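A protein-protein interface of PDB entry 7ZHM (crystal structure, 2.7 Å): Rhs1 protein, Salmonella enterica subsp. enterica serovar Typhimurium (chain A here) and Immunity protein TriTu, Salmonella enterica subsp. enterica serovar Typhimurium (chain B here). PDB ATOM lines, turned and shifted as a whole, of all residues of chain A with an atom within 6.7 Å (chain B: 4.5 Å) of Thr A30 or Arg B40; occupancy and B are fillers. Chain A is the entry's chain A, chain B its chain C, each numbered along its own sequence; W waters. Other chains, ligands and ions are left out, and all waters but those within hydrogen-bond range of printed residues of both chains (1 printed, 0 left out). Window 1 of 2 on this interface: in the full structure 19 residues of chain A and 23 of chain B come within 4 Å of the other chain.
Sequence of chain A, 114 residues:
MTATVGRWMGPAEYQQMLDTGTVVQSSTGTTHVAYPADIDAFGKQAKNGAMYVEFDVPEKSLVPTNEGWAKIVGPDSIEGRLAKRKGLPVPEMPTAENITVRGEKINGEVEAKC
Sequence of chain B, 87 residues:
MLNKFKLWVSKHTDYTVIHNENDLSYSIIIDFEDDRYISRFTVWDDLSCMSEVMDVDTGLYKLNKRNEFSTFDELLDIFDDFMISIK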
ATOM      1  N   ARG A   7     -12.366  18.051   8.341  1.00  0.00           N
ATOM      2  CA  ARG A   7     -12.659  16.631   8.674  1.00  0.00           C
ATOM      3  C   ARG A   7     -11.364  15.888   9.010  1.00  0.00           C
ATOM      4  O   ARG A   7     -10.435  15.918   8.192  1.00  0.00           O
ATOM      5  CB  ARG A   7     -13.390  15.938   7.517  1.00  0.00           C
ATOM      6  CG  ARG A   7     -13.918  14.558   7.879  1.00  0.00           C
ATOM      7  CD  ARG A   7     -14.856  13.962   6.848  1.00  0.00           C
ATOM      8  NE  ARG A   7     -14.834  12.506   6.914  1.00  0.00           N
ATOM      9  CZ  ARG A   7     -15.415  11.766   7.861  1.00  0.00           C
ATOM     10  NH1 ARG A   7     -16.093  12.335   8.845  1.00  0.00           N
ATOM     11  NH2 ARG A   7     -15.322  10.448   7.814  1.00  0.00           N
ATOM     12  N   VAL A  24     -15.962  11.627   0.327  1.00  0.00           N
ATOM     13  CA  VAL A  24     -16.229  10.209   0.526  1.00  0.00           C
ATOM     14  C   VAL A  24     -17.359  10.060   1.540  1.00  0.00           C
ATOM     15  O   VAL A  24     -17.352  10.709   2.579  1.00  0.00           O
ATOM     16  CB  VAL A  24     -14.987   9.450   1.024  1.00  0.00           C
ATOM     17  CG1 VAL A  24     -15.314   7.985   1.289  1.00  0.00           C
ATOM     18  CG2 VAL A  24     -13.858   9.564   0.018  1.00  0.00           C
ATOM     19  N   GLN A  25     -18.335   9.205   1.215  1.00  0.00           N
ATOM     20  CA  GLN A  25     -19.429   8.885   2.115  1.00  0.00           C
ATOM     21  C   GLN A  25     -18.924   7.937   3.195  1.00  0.00           C
ATOM     22  O   GLN A  25     -18.404   6.870   2.895  1.00  0.00           O
ATOM     23  CB  GLN A  25     -20.592   8.240   1.362  1.00  0.00           C
ATOM     24  CG  GLN A  25     -21.846   8.079   2.210  1.00  0.00           C
ATOM     25  CD  GLN A  25     -23.054   7.641   1.413  1.00  0.00           C
ATOM     26  OE1 GLN A  25     -24.057   8.355   1.333  1.00  0.00           O
ATOM     27  NE2 GLN A  25     -22.969   6.464   0.821  1.00  0.00           N
ATOM     28  N   SER A  26     -19.082   8.345   4.456  1.00  0.00           N
ATOM     29  CA  SER A  26     -18.781   7.503   5.600  1.00  0.00           C
ATOM     30  C   SER A  26     -19.493   6.161   5.459  1.00  0.00           C
ATOM     31  O   SER A  26     -20.588   6.092   4.913  1.00  0.00           O
ATOM     32  CB  SER A  26     -19.222   8.194   6.894  1.00  0.00           C
ATOM     33  OG  SER A  26     -19.038   7.344   8.015  1.00  0.00           O
ATOM     34  N   SER A  27     -18.867   5.097   5.969  1.00  0.00           N
ATOM     35  CA  SER A  27     -19.486   3.774   6.009  1.00  0.00           C
ATOM     36  C   SER A  27     -20.637   3.708   7.031  1.00  0.00           C
ATOM     37  O   SER A  27     -21.335   2.696   7.114  1.00  0.00           O
ATOM     38  CB  SER A  27     -18.440   2.683   6.278  1.00  0.00           C
ATOM     39  OG  SER A  27     -17.606   3.013   7.375  1.00  0.00           O
ATOM     40  N   THR A  28     -20.825   4.794   7.795  1.00  0.00           N
ATOM     41  CA  THR A  28     -22.001   4.974   8.645  1.00  0.00           C
ATOM     42  C   THR A  28     -23.229   5.445   7.861  1.00  0.00           C
ATOM     43  O   THR A  28     -24.356   5.333   8.353  1.00  0.00           O
ATOM     44  CB  THR A  28     -21.755   5.986   9.787  1.00  0.00           C
ATOM     45  OG1 THR A  28     -21.542   7.299   9.248  1.00  0.00           O
ATOM     46  CG2 THR A  28     -20.568   5.566  10.634  1.00  0.00           C
ATOM     47  N   GLY A  29     -22.998   5.990   6.660  1.00  0.00           N
ATOM     48  CA  GLY A  29     -24.051   6.496   5.792  1.00  0.00           C
ATOM     49  C   GLY A  29     -24.087   8.012   5.718  1.00  0.00           C
ATOM     50  O   GLY A  29     -24.578   8.575   4.743  1.00  0.00           O
ATOM     51  N   THR A  30     -23.562   8.667   6.761  1.00  0.00           N
ATOM     52  CA  THR A  30     -23.502  10.119   6.846  1.00  0.00           C
ATOM     53  C   THR A  30     -22.092  10.564   7.241  1.00  0.00           C
ATOM     54  O   THR A  30     -21.561  10.160   8.276  1.00  0.00           O
ATOM     55  CB  THR A  30     -24.516  10.663   7.875  1.00  0.00           C
ATOM     56  OG1 THR A  30     -25.778  10.005   7.710  1.00  0.00           O
ATOM     57  CG2 THR A  30     -24.706  12.165   7.705  1.00  0.00           C
ATOM     58  N   THR A  31     -21.491  11.402   6.395  1.00  0.00           N
ATOM     59  CA  THR A  31     -20.190  11.981   6.661  1.00  0.00           C
ATOM     60  C   THR A  31     -20.384  13.242   7.487  1.00  0.00           C
ATOM     61  O   THR A  31     -21.121  14.141   7.094  1.00  0.00           O
ATOM     62  CB  THR A  31     -19.455  12.306   5.348  1.00  0.00           C
ATOM     63  OG1 THR A  31     -19.313  11.105   4.584  1.00  0.00           O
ATOM     64  CG2 THR A  31     -18.075  12.892   5.625  1.00  0.00           C
ATOM     65  N   HIS A  32     -19.726  13.290   8.648  1.00  0.00           N
ATOM     66  CA  HIS A  32     -19.774  14.438   9.536  1.00  0.00           C
ATOM     67  C   HIS A  32     -18.524  15.277   9.315  1.00  0.00           C
ATOM     68  O   HIS A  32     -17.454  14.742   9.041  1.00  0.00           O
ATOM     69  CB  HIS A  32     -19.881  13.979  10.990  1.00  0.00           C
ATOM     70  CG  HIS A  32     -21.221  13.411  11.343  1.00  0.00           C
ATOM     71  ND1 HIS A  32     -21.640  13.247  12.644  1.00  0.00           N
ATOM     72  CD2 HIS A  32     -22.243  12.984  10.564  1.00  0.00           C
ATOM     73  CE1 HIS A  32     -22.858  12.737  12.652  1.00  0.00           C
ATOM     74  NE2 HIS A  32     -23.245  12.563  11.402  1.00  0.00           N
ATOM     75  N   TRP A  69     -20.530  21.132  14.318  1.00  0.00           N
ATOM     76  CA  TRP A  69     -20.453  20.113  13.269  1.00  0.00           C
ATOM     77  C   TRP A  69     -21.667  20.164  12.349  1.00  0.00           C
ATOM     78  O   TRP A  69     -22.661  20.817  12.655  1.00  0.00           O
ATOM     79  CB  TRP A  69     -20.305  18.704  13.864  1.00  0.00           C
ATOM     80  CG  TRP A  69     -21.464  18.262  14.699  1.00  0.00           C
ATOM     81  CD1 TRP A  69     -21.692  18.556  16.014  1.00  0.00           C
ATOM     82  CD2 TRP A  69     -22.551  17.435  14.281  1.00  0.00           C
ATOM     83  NE1 TRP A  69     -22.859  17.969  16.439  1.00  0.00           N
ATOM     84  CE2 TRP A  69     -23.407  17.273  15.394  1.00  0.00           C
ATOM     85  CE3 TRP A  69     -22.888  16.810  13.071  1.00  0.00           C
ATOM     86  CZ2 TRP A  69     -24.577  16.522  15.332  1.00  0.00           C
ATOM     87  CZ3 TRP A  69     -24.053  16.056  13.012  1.00  0.00           C
ATOM     88  CH2 TRP A  69     -24.887  15.926  14.133  1.00  0.00           C
ATOM     89  N   ALA A  70     -21.563  19.462  11.216  1.00  0.00           N
ATOM     90  CA  ALA A  70     -22.597  19.426  10.191  1.00  0.00           C
ATOM     91  C   ALA A  70     -22.622  18.074   9.503  1.00  0.00           C
ATOM     92  O   ALA A  70     -21.611  17.363   9.482  1.00  0.00           O
ATOM     93  CB  ALA A  70     -22.352  20.523   9.165  1.00  0.00           C
ATOM     94  N   LYS A  71     -23.788  17.728   8.945  1.00  0.00           N
ATOM     95  CA  LYS A  71     -23.955  16.544   8.102  1.00  0.00           C
ATOM     96  C   LYS A  71     -23.747  16.921   6.643  1.00  0.00           C
ATOM     97  O   LYS A  71     -24.156  17.993   6.218  1.00  0.00           O
ATOM     98  CB  LYS A  71     -25.355  15.954   8.259  1.00  0.00           C
ATOM     99  CG  LYS A  71     -25.639  15.386   9.633  1.00  0.00           C
ATOM    100  CD  LYS A  71     -27.038  14.795   9.719  1.00  0.00           C
ATOM    101  CE  LYS A  71     -27.463  14.539  11.159  1.00  0.00           C
ATOM    102  NZ  LYS A  71     -28.851  14.005  11.204  1.00  0.00           N
ATOM    103  N   ILE A  72     -23.103  16.032   5.885  1.00  0.00           N
ATOM    104  CA  ILE A  72     -23.092  16.109   4.434  1.00  0.00           C
ATOM    105  C   ILE A  72     -24.136  15.112   3.936  1.00  0.00           C
ATOM    106  O   ILE A  72     -24.084  13.932   4.273  1.00  0.00           O
ATOM    107  CB  ILE A  72     -21.695  15.830   3.845  1.00  0.00           C
ATOM    108  CG1 ILE A  72     -20.775  17.013   4.156  1.00  0.00           C
ATOM    109  CG2 ILE A  72     -21.781  15.615   2.335  1.00  0.00           C
ATOM    110  CD1 ILE A  72     -19.329  16.824   3.767  1.00  0.00           C
ATOM    111  N   VAL A  73     -25.096  15.615   3.155  1.00  0.00           N
ATOM    112  CA  VAL A  73     -26.230  14.846   2.653  1.00  0.00           C
ATOM    113  C   VAL A  73     -25.833  14.044   1.410  1.00  0.00           C
ATOM    114  O   VAL A  73     -25.655  14.607   0.323  1.00  0.00           O
ATOM    115  CB  VAL A  73     -27.404  15.792   2.313  1.00  0.00           C
ATOM    116  CG1 VAL A  73     -28.489  15.061   1.540  1.00  0.00           C
ATOM    117  CG2 VAL A  73     -27.963  16.429   3.579  1.00  0.00           C
ATOM    118  N   GLY A  74     -25.688  12.728   1.587  1.00  0.00           N
ATOM    119  CA  GLY A  74     -25.358  11.803   0.516  1.00  0.00           C
ATOM    120  C   GLY A  74     -26.508  10.835   0.255  1.00  0.00           C
ATOM    121  O   GLY A  74     -27.568  10.958   0.862  1.00  0.00           O
ATOM    122  N   PRO A  75     -26.336   9.856  -0.661  1.00  0.00           N
ATOM    123  CA  PRO A  75     -27.375   8.865  -0.950  1.00  0.00           C
ATOM    124  C   PRO A  75     -27.889   8.099   0.279  1.00  0.00           C
ATOM    125  O   PRO A  75     -29.079   7.852   0.352  1.00  0.00           O
ATOM    126  CB  PRO A  75     -26.679   7.891  -1.914  1.00  0.00           C
ATOM    127  CG  PRO A  75     -25.620   8.731  -2.588  1.00  0.00           C
ATOM    128  CD  PRO A  75     -25.148   9.688  -1.515  1.00  0.00           C
ATOM    129  N   ASP A  76     -26.987   7.742   1.198  1.00  0.00           N
ATOM    130  CA  ASP A  76     -27.309   6.881   2.330  1.00  0.00           C
ATOM    131  C   ASP A  76     -27.508   7.638   3.646  1.00  0.00           C
ATOM    132  O   ASP A  76     -27.718   7.022   4.691  1.00  0.00           O
ATOM    133  CB  ASP A  76     -26.242   5.797   2.466  1.00  0.00           C
ATOM    134  CG  ASP A  76     -26.362   4.743   1.381  1.00  0.00           C
ATOM    135  OD1 ASP A  76     -27.360   3.988   1.403  1.00  0.00           O
ATOM    136  OD2 ASP A  76     -25.476   4.681   0.496  1.00  0.00           O
ATOM    137  N   SER A  77     -27.470   8.974   3.586  1.00  0.00           N
ATOM    138  CA  SER A  77     -27.885   9.817   4.700  1.00  0.00           C
ATOM    139  C   SER A  77     -29.390   9.659   4.885  1.00  0.00           C
ATOM    140  O   SER A  77     -30.089   9.231   3.964  1.00  0.00           O
ATOM    141  CB  SER A  77     -27.547  11.279   4.424  1.00  0.00           C
ATOM    142  OG  SER A  77     -28.325  11.799   3.357  1.00  0.00           O
ATOM    143  N   ILE A  78     -29.884  10.014   6.075  1.00  0.00           N
ATOM    144  CA  ILE A  78     -31.310   9.935   6.377  1.00  0.00           C
ATOM    145  C   ILE A  78     -32.126  10.766   5.381  1.00  0.00           C
ATOM    146  O   ILE A  78     -33.162  10.312   4.903  1.00  0.00           O
ATOM    147  CB  ILE A  78     -31.609  10.380   7.825  1.00  0.00           C
ATOM    148  CG1 ILE A  78     -31.017   9.377   8.816  1.00  0.00           C
ATOM    149  CG2 ILE A  78     -33.109  10.522   8.062  1.00  0.00           C
ATOM    150  CD1 ILE A  78     -31.596   7.975   8.733  1.00  0.00           C
ATOM    151  N   ARG A  81     -32.223   8.841   2.066  1.00  0.00           N
ATOM    152  CA  ARG A  81     -33.145   7.672   2.136  1.00  0.00           C
ATOM    153  C   ARG A  81     -34.600   8.154   2.071  1.00  0.00           C
ATOM    154  O   ARG A  81     -35.435   7.419   1.505  1.00  0.00           O
ATOM    155  CB  ARG A  81     -32.890   6.851   3.405  1.00  0.00           C
ATOM    156  CG  ARG A  81     -31.594   6.053   3.381  1.00  0.00           C
ATOM    157  CD  ARG A  81     -31.600   4.931   2.361  1.00  0.00           C
ATOM    158  NE  ARG A  81     -30.359   4.168   2.399  1.00  0.00           N
ATOM    159  CZ  ARG A  81     -30.049   3.246   3.307  1.00  0.00           C
ATOM    160  NH1 ARG A  81     -30.891   2.946   4.284  1.00  0.00           N
ATOM    161  NH2 ARG A  81     -28.886   2.623   3.238  1.00  0.00           N
ATOM    162  N   MET A  93     -22.958  12.706  -3.254  1.00  0.00           N
ATOM    163  CA  MET A  93     -21.918  13.314  -2.441  1.00  0.00           C
ATOM    164  C   MET A  93     -21.388  14.519  -3.212  1.00  0.00           C
ATOM    165  O   MET A  93     -21.146  14.430  -4.416  1.00  0.00           O
ATOM    166  CB  MET A  93     -20.792  12.324  -2.150  1.00  0.00           C
ATOM    167  CG  MET A  93     -21.194  11.120  -1.299  1.00  0.00           C
ATOM    168  SD  MET A  93     -21.788  11.536   0.350  1.00  0.00           S
ATOM    169  CE  MET A  93     -20.361  12.334   1.063  1.00  0.00           C
ATOM    170  N   ILE B  30     -27.364   0.658  13.250  1.00  0.00           N
ATOM    171  CA  ILE B  30     -28.624  -0.069  13.241  1.00  0.00           C
ATOM    172  C   ILE B  30     -29.645   0.726  12.420  1.00  0.00           C
ATOM    173  O   ILE B  30     -30.174   1.730  12.890  1.00  0.00           O
ATOM    174  CB  ILE B  30     -29.125  -0.331  14.674  1.00  0.00           C
ATOM    175  CG1 ILE B  30     -28.142  -1.260  15.400  1.00  0.00           C
ATOM    176  CG2 ILE B  30     -30.521  -0.940  14.650  1.00  0.00           C
ATOM    177  CD1 ILE B  30     -28.404  -1.403  16.887  1.00  0.00           C
ATOM    178  N   ASP B  31     -29.871   0.276  11.178  1.00  0.00           N
ATOM    179  CA  ASP B  31     -30.897   0.809  10.290  1.00  0.00           C
ATOM    180  C   ASP B  31     -32.230   0.143  10.598  1.00  0.00           C
ATOM    181  O   ASP B  31     -32.310  -1.081  10.671  1.00  0.00           O
ATOM    182  CB  ASP B  31     -30.553   0.519   8.820  1.00  0.00           C
ATOM    183  CG  ASP B  31     -29.611   1.542   8.211  1.00  0.00           C
ATOM    184  OD1 ASP B  31     -29.670   2.731   8.581  1.00  0.00           O
ATOM    185  OD2 ASP B  31     -28.821   1.153   7.328  1.00  0.00           O
ATOM    186  N   SER B  39     -35.117   5.429  10.254  1.00  0.00           N
ATOM    187  CA  SER B  39     -34.283   5.655  11.429  1.00  0.00           C
ATOM    188  C   SER B  39     -32.956   4.920  11.374  1.00  0.00           C
ATOM    189  O   SER B  39     -32.801   3.936  10.653  1.00  0.00           O
ATOM    190  CB  SER B  39     -35.032   5.228  12.686  1.00  0.00           C
ATOM    191  OG  SER B  39     -35.299   3.837  12.647  1.00  0.00           O
ATOM    192  N   ARG B  40     -31.995   5.418  12.155  1.00  0.00           N
ATOM    193  CA  ARG B  40     -30.624   4.858  12.253  1.00  0.00           C
ATOM    194  C   ARG B  40     -30.010   5.239  13.602  1.00  0.00           C
ATOM    195  O   ARG B  40     -30.134   6.414  14.008  1.00  0.00           O
ATOM    196  CB  ARG B  40     -29.735   5.367  11.114  1.00  0.00           C
ATOM    197  CG  ARG B  40     -28.356   4.726  11.072  1.00  0.00           C
ATOM    198  CD  ARG B  40     -27.503   5.283   9.952  1.00  0.00           C
ATOM    199  NE  ARG B  40     -28.044   4.935   8.644  1.00  0.00           N
ATOM    200  CZ  ARG B  40     -28.022   5.720   7.566  1.00  0.00           C
ATOM    201  NH1 ARG B  40     -27.487   6.930   7.622  1.00  0.00           N
ATOM    202  NH2 ARG B  40     -28.558   5.293   6.434  1.00  0.00           N
ATOM    203  N   PHE B  41     -29.377   4.268  14.259  1.00  0.00           N
ATOM    204  CA  PHE B  41     -28.589   4.518  15.443  1.00  0.00           C
ATOM    205  C   PHE B  41     -27.145   4.158  15.104  1.00  0.00           C
ATOM    206  O   PHE B  41     -26.863   3.034  14.699  1.00  0.00           O
ATOM    207  CB  PHE B  41     -29.112   3.700  16.622  1.00  0.00           C
ATOM    208  CG  PHE B  41     -28.349   3.932  17.882  1.00  0.00           C
ATOM    209  CD1 PHE B  41     -28.531   5.102  18.604  1.00  0.00           C
ATOM    210  CD2 PHE B  41     -27.427   2.997  18.334  1.00  0.00           C
ATOM    211  CE1 PHE B  41     -27.810   5.332  19.759  1.00  0.00           C
ATOM    212  CE2 PHE B  41     -26.704   3.221  19.490  1.00  0.00           C
ATOM    213  CZ  PHE B  41     -26.897   4.390  20.206  1.00  0.00           C
ATOM    214  N   THR B  42     -26.246   5.135  15.244  1.00  0.00           N
ATOM    215  CA  THR B  42     -24.824   4.945  15.007  1.00  0.00           C
ATOM    216  C   THR B  42     -24.079   5.114  16.320  1.00  0.00           C
ATOM    217  O   THR B  42     -24.308   6.080  17.041  1.00  0.00           O
ATOM    218  CB  THR B  42     -24.268   5.966  13.996  1.00  0.00           C
ATOM    219  OG1 THR B  42     -25.080   5.970  12.811  1.00  0.00           O
ATOM    220  CG2 THR B  42     -22.829   5.616  13.625  1.00  0.00           C
ATOM    221  N   MET B  50     -24.903   8.607  17.620  1.00  0.00           N
ATOM    222  CA  MET B  50     -25.839   9.452  16.899  1.00  0.00           C
ATOM    223  C   MET B  50     -27.192   8.748  16.802  1.00  0.00           C
ATOM    224  O   MET B  50     -27.253   7.575  16.443  1.00  0.00           O
ATOM    225  CB  MET B  50     -25.294   9.736  15.504  1.00  0.00           C
ATOM    226  CG  MET B  50     -26.102  10.749  14.713  1.00  0.00           C
ATOM    227  SD  MET B  50     -25.930  12.408  15.380  1.00  0.00           S
ATOM    228  CE  MET B  50     -27.406  13.194  14.736  1.00  0.00           C
ATOM    229  N   SER B  51     -28.264   9.475  17.138  1.00  0.00           N
ATOM    230  CA  SER B  51     -29.634   8.965  17.093  1.00  0.00           C
ATOM    231  C   SER B  51     -30.459   9.757  16.085  1.00  0.00           C
ATOM    232  O   SER B  51     -30.716  10.943  16.289  1.00  0.00           O
ATOM    233  CB  SER B  51     -30.287   9.061  18.471  1.00  0.00           C
ATOM    234  OG  SER B  51     -29.546   8.334  19.427  1.00  0.00           O
ATOM    235  N   GLU B  52     -30.876   9.085  15.005  1.00  0.00           N
ATOM    236  CA  GLU B  52     -31.652   9.691  13.929  1.00  0.00           C
ATOM    237  C   GLU B  52     -32.975   8.950  13.702  1.00  0.00           C
ATOM    238  O   GLU B  52     -32.977   7.747  13.432  1.00  0.00           O
ATOM    239  CB  GLU B  52     -30.837   9.698  12.640  1.00  0.00           C
ATOM    240  CG  GLU B  52     -29.579  10.557  12.705  1.00  0.00           C
ATOM    241  CD  GLU B  52     -28.670  10.373  11.494  1.00  0.00           C
ATOM    242  OE1 GLU B  52     -28.186   9.238  11.272  1.00  0.00           O
ATOM    243  OE2 GLU B  52     -28.425  11.367  10.773  1.00  0.00           O
ATOM    244  N   PHE B  82     -33.783   6.128  21.843  1.00  0.00           N
ATOM    245  CA  PHE B  82     -33.916   5.803  20.424  1.00  0.00           C
ATOM    246  C   PHE B  82     -34.952   4.700  20.180  1.00  0.00           C
ATOM    247  O   PHE B  82     -35.792   4.831  19.299  1.00  0.00           O
ATOM    248  CB  PHE B  82     -32.556   5.405  19.840  1.00  0.00           C
ATOM    249  CG  PHE B  82     -32.628   4.904  18.427  1.00  0.00           C
ATOM    250  CD1 PHE B  82     -32.654   5.795  17.364  1.00  0.00           C
ATOM    251  CD2 PHE B  82     -32.672   3.544  18.159  1.00  0.00           C
ATOM    252  CE1 PHE B  82     -32.721   5.338  16.058  1.00  0.00           C
ATOM    253  CE2 PHE B  82     -32.744   3.079  16.857  1.00  0.00           C
ATOM    254  CZ  PHE B  82     -32.768   3.978  15.806  1.00  0.00           C
HETATM  255  O   HOH W   1     -28.156  11.241   8.010  1.00  0.00           O
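NH2 of Arg B40 sits at hydrogen-bond distance from O of Asp A76, at 2.6 Å. NZ of Lys A71 lies within salt-bridge range of OE2 of Glu B52 (2.7 Å).
Among the printed residues, merely in contact across the chains: Thr A28 with Arg B40 (3.5 Å), Thr A28 with Thr B42 (3.7 Å), Gly A29 with Arg B40 (3.9 Å), Thr A30 with Arg B40 (3.5 Å), Trp A69 with Met B50 (3.8 Å), Lys A71 with Met B50 (3.8 Å), Ile A78 with Arg B40 (3.99 Å), Ile A78 with Glu B52 (3.7 Å) and Arg A81 with Arg B40 (3.9 Å).
Of chain B, only Arg B40 comes within 4 Å of Thr A30. Of the printed residues of chain A, Arg B40 touches Thr A28, Gly A29, Thr A30, Asp A76, Ile A78 and Arg A81. Of the printed residues of chain B, Lys A71 touches Met B50 and Glu B52. Of the printed residues of chain B, Arg A81 touches Arg B40 (3.9 Å). The nearest residue of chain B that does not touch Thr A30 is Glu B52 (4.3 Å). The nearest printed residue of chain B that does not touch Gly A29 is Thr B42 (6.5 Å).
Water W1 lies within hydrogen-bond range of OG1 of Thr A30 (2.7 Å), OE2 of Glu B52 (2.8 Å) and N of Ile A78 (2.9 Å).
OG1 of Thr A28 is in hydrogen-bond range of O of Thr A30 (3.0 Å). The side-chain hydroxyl (OG) of Ser A26 is in hydrogen-bond range of the side-chain hydroxyl (OG1) of Thr A28 (2.8 Å). OE1 of Gln A25 lies within hydrogen-bond range of N of Asp A76 (3.0 Å). OD1 of Asp A76 lies within salt-bridge range of NH2 of Arg A81 (2.7 Å). The guanidinium group of Arg B40 is in salt-bridge range of the side-chain carboxylate of Asp B31. The backbone carbonyl oxygen (O) of Gly A29 sits at hydrogen-bond distance from the backbone NH (N) of Ser A77.
Of the 10 printed residues of chain B, 4 touch a printed residue of chain A. Printed residues of chain A that touch a printed residue of chain B: Thr A28, Gly A29, Thr A30, Trp A69, Lys A71, Asp A76, Ile A78 and Arg A81. Hydrophobic or aromatic side chains of chain A that line the printed part of chain B: Trp A69 and Ile A78.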
